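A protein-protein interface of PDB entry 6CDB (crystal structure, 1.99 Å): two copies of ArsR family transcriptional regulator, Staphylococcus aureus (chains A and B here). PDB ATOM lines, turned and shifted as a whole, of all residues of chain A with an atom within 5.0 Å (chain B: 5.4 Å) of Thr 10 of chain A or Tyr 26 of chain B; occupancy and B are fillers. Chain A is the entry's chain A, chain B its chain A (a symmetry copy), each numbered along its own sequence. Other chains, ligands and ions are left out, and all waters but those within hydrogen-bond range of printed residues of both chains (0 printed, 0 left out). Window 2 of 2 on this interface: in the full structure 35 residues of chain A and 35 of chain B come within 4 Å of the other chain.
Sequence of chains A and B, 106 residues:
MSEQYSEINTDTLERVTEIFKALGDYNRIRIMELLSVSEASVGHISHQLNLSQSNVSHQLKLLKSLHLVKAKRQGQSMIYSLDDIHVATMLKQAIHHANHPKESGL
OD1 of Asp 25 of chain B is in salt-bridge range of NH1 of Arg 28 of chain B (3.6 Å). O of Leu 13 of chain A lies within hydrogen-bond range of OG1 of Thr 17 of chain A (2.7 Å). The side-chain carboxylate of Asp 25 of chain B lies within hydrogen-bond range of the backbone NH of Asn 27 of chain B (3.1 Å). The side-chain amide oxygen of Asn 27 of chain B is in hydrogen-bond range of the guanidinium group of Arg 30 of chain B, 3.2 Å away.
Among the printed residues, pairs that only touch across the chains: Glu 14 of chain A with Tyr 26 of chain B, Thr 10 of chain A with Tyr 26 of chain B, Thr 17 of chain A with Tyr 26 of chain B, Thr 17 of chain A with Ile 29 of chain B, Leu 13 of chain A with Arg 30 of chain B and Thr 17 of chain A with Asp 25 of chain B.
Of chain B, only Tyr 26 (3.2 Å) comes within 4 Å of Thr 10 of chain A. Tyr 26 of chain B touches just these residues of chain A: Thr 10 (3.2 Å), Glu 14 (3.2 Å) and Thr 17 (3.4 Å). Printed residues of chain A within 4 Å of Ile 29 of chain B: Thr 17 (3.8 Å). Printed residues of chain B within 4 Å of Leu 13 of chain A: Arg 30 (3.9 Å). Of the printed residues of chain B, Thr 17 of chain A touches Asp 25 (3.9 Å), Tyr 26 (3.4 Å) and Ile 29 (3.8 Å). Printed residues of chain B within 4 Å of Glu 14 of chain A: Tyr 26. Of the printed residues of chain A, Arg 30 of chain B touches Leu 13 (3.9 Å). Ile 8 of chain A touches none of the printed residues of chain B. Thr 12 of chain A touches none of the printed residues of chain B. The nearest printed residue of chain B that does not touch Thr 10 of chain A is Arg 30 of chain B (6.3 Å).
Hydrophobic or aromatic side chains of chain A within 4 Å of the printed part of chain B: Leu 13. Among the printed residues, no Asp or Glu carboxylate lies within 4 Å of a Lys or Arg side-chain nitrogen of the other chain.
No position is printed for both chains. Of the 6 pairs that touch across the chains among the printed residues, none has its exchanged pair printed and touching as well.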
ATOM      1  N   ILE A   8      12.677  13.207 -19.750  1.00  0.00           N
ATOM      2  CA  ILE A   8      13.864  13.131 -20.613  1.00  0.00           C
ATOM      3  C   ILE A   8      14.080  11.649 -20.919  1.00  0.00           C
ATOM      4  O   ILE A   8      14.675  10.891 -20.148  1.00  0.00           O
ATOM      5  CB  ILE A   8      15.090  13.804 -19.984  1.00  0.00           C
ATOM      6  CG1 ILE A   8      15.105  15.310 -20.307  1.00  0.00           C
ATOM      7  CG2 ILE A   8      16.408  13.175 -20.482  1.00  0.00           C
ATOM      8  CD1 ILE A   8      14.026  16.144 -19.622  1.00  0.00           C
ATOM      9  N   ASN A   9      13.543  11.224 -22.045  1.00  0.00           N
ATOM     10  CA  ASN A   9      13.793   9.898 -22.572  1.00  0.00           C
ATOM     11  C   ASN A   9      14.571  10.029 -23.879  1.00  0.00           C
ATOM     12  O   ASN A   9      14.833  11.136 -24.368  1.00  0.00           O
ATOM     13  CB  ASN A   9      12.479   9.137 -22.763  1.00  0.00           C
ATOM     14  CG  ASN A   9      11.541   9.837 -23.724  1.00  0.00           C
ATOM     15  OD1 ASN A   9      11.242  11.022 -23.563  1.00  0.00           O
ATOM     16  ND2 ASN A   9      11.085   9.115 -24.740  1.00  0.00           N
ATOM     17  N   THR A  10      14.938   8.876 -24.434  1.00  0.00           N
ATOM     18  CA  THR A  10      15.754   8.840 -25.642  1.00  0.00           C
ATOM     19  C   THR A  10      15.108   9.617 -26.783  1.00  0.00           C
ATOM     20  O   THR A  10      15.781  10.399 -27.469  1.00  0.00           O
ATOM     21  CB  THR A  10      15.997   7.383 -26.045  1.00  0.00           C
ATOM     22  OG1 THR A  10      16.835   6.757 -25.066  1.00  0.00           O
ATOM     23  CG2 THR A  10      16.653   7.288 -27.426  1.00  0.00           C
ATOM     24  N   ASP A  11      13.803   9.415 -26.997  1.00  0.00           N
ATOM     25  CA  ASP A  11      13.086  10.123 -28.059  1.00  0.00           C
ATOM     26  C   ASP A  11      13.238  11.635 -27.925  1.00  0.00           C
ATOM     27  O   ASP A  11      13.525  12.333 -28.909  1.00  0.00           O
ATOM     28  CB  ASP A  11      11.605   9.736 -28.031  1.00  0.00           C
ATOM     29  CG  ASP A  11      11.397   8.234 -27.891  1.00  0.00           C
ATOM     30  OD1 ASP A  11      10.551   7.819 -27.059  1.00  0.00           O
ATOM     31  OD2 ASP A  11      12.084   7.472 -28.612  1.00  0.00           O
ATOM     32  N   THR A  12      13.041  12.161 -26.712  1.00  0.00           N
ATOM     33  CA  THR A  12      13.190  13.596 -26.495  1.00  0.00           C
ATOM     34  C   THR A  12      14.553  14.083 -26.963  1.00  0.00           C
ATOM     35  O   THR A  12      14.650  15.073 -27.696  1.00  0.00           O
ATOM     36  CB  THR A  12      12.994  13.949 -25.019  1.00  0.00           C
ATOM     37  OG1 THR A  12      11.736  13.442 -24.559  1.00  0.00           O
ATOM     38  CG2 THR A  12      13.020  15.471 -24.849  1.00  0.00           C
ATOM     39  N   LEU A  13      15.625  13.404 -26.537  1.00  0.00           N
ATOM     40  CA  LEU A  13      16.962  13.874 -26.888  1.00  0.00           C
ATOM     41  C   LEU A  13      17.240  13.702 -28.375  1.00  0.00           C
ATOM     42  O   LEU A  13      18.009  14.475 -28.952  1.00  0.00           O
ATOM     43  CB  LEU A  13      18.021  13.155 -26.045  1.00  0.00           C
ATOM     44  CG  LEU A  13      17.964  13.414 -24.525  1.00  0.00           C
ATOM     45  CD1 LEU A  13      19.244  12.948 -23.833  1.00  0.00           C
ATOM     46  CD2 LEU A  13      17.680  14.896 -24.217  1.00  0.00           C
ATOM     47  N   GLU A  14      16.622  12.715 -29.018  1.00  0.00           N
ATOM     48  CA  GLU A  14      16.744  12.630 -30.466  1.00  0.00           C
ATOM     49  C   GLU A  14      16.093  13.830 -31.148  1.00  0.00           C
ATOM     50  O   GLU A  14      16.692  14.433 -32.050  1.00  0.00           O
ATOM     51  CB  GLU A  14      16.141  11.321 -30.963  1.00  0.00           C
ATOM     52  CG  GLU A  14      16.919  10.090 -30.497  1.00  0.00           C
ATOM     53  CD  GLU A  14      17.706   9.465 -31.628  1.00  0.00           C
ATOM     54  OE1 GLU A  14      17.082   8.763 -32.458  1.00  0.00           O
ATOM     55  OE2 GLU A  14      18.937   9.696 -31.698  1.00  0.00           O
ATOM     56  N   THR A  17      18.261  16.723 -30.712  1.00  0.00           N
ATOM     57  CA  THR A  17      19.330  16.595 -31.693  1.00  0.00           C
ATOM     58  C   THR A  17      18.893  17.095 -33.067  1.00  0.00           C
ATOM     59  O   THR A  17      19.654  17.792 -33.747  1.00  0.00           O
ATOM     60  CB  THR A  17      19.794  15.137 -31.766  1.00  0.00           C
ATOM     61  OG1 THR A  17      20.241  14.716 -30.473  1.00  0.00           O
ATOM     62  CG2 THR A  17      20.939  14.975 -32.762  1.00  0.00           C
ATOM     63  N   GLY B  24      24.544  19.623 -32.802  1.00  0.00           N
ATOM     64  CA  GLY B  24      23.749  18.731 -33.624  1.00  0.00           C
ATOM     65  C   GLY B  24      24.328  17.321 -33.624  1.00  0.00           C
ATOM     66  O   GLY B  24      24.670  16.783 -34.675  1.00  0.00           O
ATOM     67  N   ASP B  25      24.441  16.715 -32.449  1.00  0.00           N
ATOM     68  CA  ASP B  25      25.110  15.423 -32.288  1.00  0.00           C
ATOM     69  C   ASP B  25      24.472  14.724 -31.098  1.00  0.00           C
ATOM     70  O   ASP B  25      24.494  15.271 -29.992  1.00  0.00           O
ATOM     71  CB  ASP B  25      26.617  15.622 -32.077  1.00  0.00           C
ATOM     72  CG  ASP B  25      27.376  14.308 -31.894  1.00  0.00           C
ATOM     73  OD1 ASP B  25      28.221  13.978 -32.748  1.00  0.00           O
ATOM     74  OD2 ASP B  25      27.153  13.614 -30.890  1.00  0.00           O
ATOM     75  N   TYR B  26      23.916  13.527 -31.322  1.00  0.00           N
ATOM     76  CA  TYR B  26      23.114  12.858 -30.292  1.00  0.00           C
ATOM     77  C   TYR B  26      23.902  12.643 -29.007  1.00  0.00           C
ATOM     78  O   TYR B  26      23.403  12.905 -27.904  1.00  0.00           O
ATOM     79  CB  TYR B  26      22.600  11.522 -30.822  1.00  0.00           C
ATOM     80  CG  TYR B  26      21.818  10.701 -29.817  1.00  0.00           C
ATOM     81  CD1 TYR B  26      20.576  11.127 -29.367  1.00  0.00           C
ATOM     82  CD2 TYR B  26      22.308   9.488 -29.353  1.00  0.00           C
ATOM     83  CE1 TYR B  26      19.847  10.390 -28.469  1.00  0.00           C
ATOM     84  CE2 TYR B  26      21.583   8.729 -28.440  1.00  0.00           C
ATOM     85  CZ  TYR B  26      20.352   9.191 -28.004  1.00  0.00           C
ATOM     86  OH  TYR B  26      19.618   8.463 -27.108  1.00  0.00           O
ATOM     87  N   ASN B  27      25.127  12.135 -29.129  1.00  0.00           N
ATOM     88  CA  ASN B  27      25.936  11.856 -27.949  1.00  0.00           C
ATOM     89  C   ASN B  27      26.367  13.136 -27.250  1.00  0.00           C
ATOM     90  O   ASN B  27      26.440  13.176 -26.016  1.00  0.00           O
ATOM     91  CB  ASN B  27      27.153  11.006 -28.334  1.00  0.00           C
ATOM     92  CG  ASN B  27      26.806   9.539 -28.472  1.00  0.00           C
ATOM     93  OD1 ASN B  27      25.887   9.050 -27.812  1.00  0.00           O
ATOM     94  ND2 ASN B  27      27.532   8.828 -29.341  1.00  0.00           N
ATOM     95  N   ARG B  28      26.672  14.185 -28.017  1.00  0.00           N
ATOM     96  CA  ARG B  28      26.987  15.471 -27.401  1.00  0.00           C
ATOM     97  C   ARG B  28      25.782  16.037 -26.662  1.00  0.00           C
ATOM     98  O   ARG B  28      25.933  16.633 -25.595  1.00  0.00           O
ATOM     99  CB  ARG B  28      27.478  16.472 -28.446  1.00  0.00           C
ATOM    100  CG  ARG B  28      28.882  16.194 -28.934  1.00  0.00           C
ATOM    101  CD  ARG B  28      29.447  17.370 -29.718  1.00  0.00           C
ATOM    102  NE  ARG B  28      30.545  16.888 -30.538  1.00  0.00           N
ATOM    103  CZ  ARG B  28      30.534  16.863 -31.860  1.00  0.00           C
ATOM    104  NH1 ARG B  28      29.499  17.365 -32.532  1.00  0.00           N
ATOM    105  NH2 ARG B  28      31.583  16.365 -32.508  1.00  0.00           N
ATOM    106  N   ILE B  29      24.580  15.862 -27.212  1.00  0.00           N
ATOM    107  CA  ILE B  29      23.379  16.265 -26.487  1.00  0.00           C
ATOM    108  C   ILE B  29      23.225  15.448 -25.204  1.00  0.00           C
ATOM    109  O   ILE B  29      22.809  15.973 -24.164  1.00  0.00           O
ATOM    110  CB  ILE B  29      22.149  16.144 -27.402  1.00  0.00           C
ATOM    111  CG1 ILE B  29      22.174  17.258 -28.464  1.00  0.00           C
ATOM    112  CG2 ILE B  29      20.853  16.193 -26.593  1.00  0.00           C
ATOM    113  CD1 ILE B  29      22.324  18.670 -27.860  1.00  0.00           C
ATOM    114  N   ARG B  30      23.570  14.157 -25.246  1.00  0.00           N
ATOM    115  CA  ARG B  30      23.454  13.345 -24.035  1.00  0.00           C
ATOM    116  C   ARG B  30      24.444  13.801 -22.971  1.00  0.00           C
ATOM    117  O   ARG B  30      24.109  13.877 -21.773  1.00  0.00           O
ATOM    118  CB  ARG B  30      23.662  11.864 -24.368  1.00  0.00           C
ATOM    119  CG  ARG B  30      22.481  11.214 -25.075  1.00  0.00           C
ATOM    120  CD  ARG B  30      22.404   9.744 -24.689  1.00  0.00           C
ATOM    121  NE  ARG B  30      23.538   9.007 -25.221  1.00  0.00           N
ATOM    122  CZ  ARG B  30      24.099   7.939 -24.652  1.00  0.00           C
ATOM    123  NH1 ARG B  30      23.650   7.451 -23.491  1.00  0.00           N
ATOM    124  NH2 ARG B  30      25.126   7.365 -25.253  1.00  0.00           N
ATOM    125  N   ILE B  31      25.669  14.107 -23.387  1.00  0.00           N
ATOM    126  CA  ILE B  31      26.654  14.652 -22.458  1.00  0.00           C
ATOM    127  C   ILE B  31      26.151  15.969 -21.869  1.00  0.00           C
ATOM    128  O   ILE B  31      26.220  16.194 -20.651  1.00  0.00           O
ATOM    129  CB  ILE B  31      28.006  14.835 -23.169  1.00  0.00           C
ATOM    130  CG1 ILE B  31      28.576  13.473 -23.604  1.00  0.00           C
ATOM    131  CG2 ILE B  31      28.980  15.620 -22.286  1.00  0.00           C
ATOM    132  CD1 ILE B  31      29.818  13.586 -24.465  1.00  0.00           C
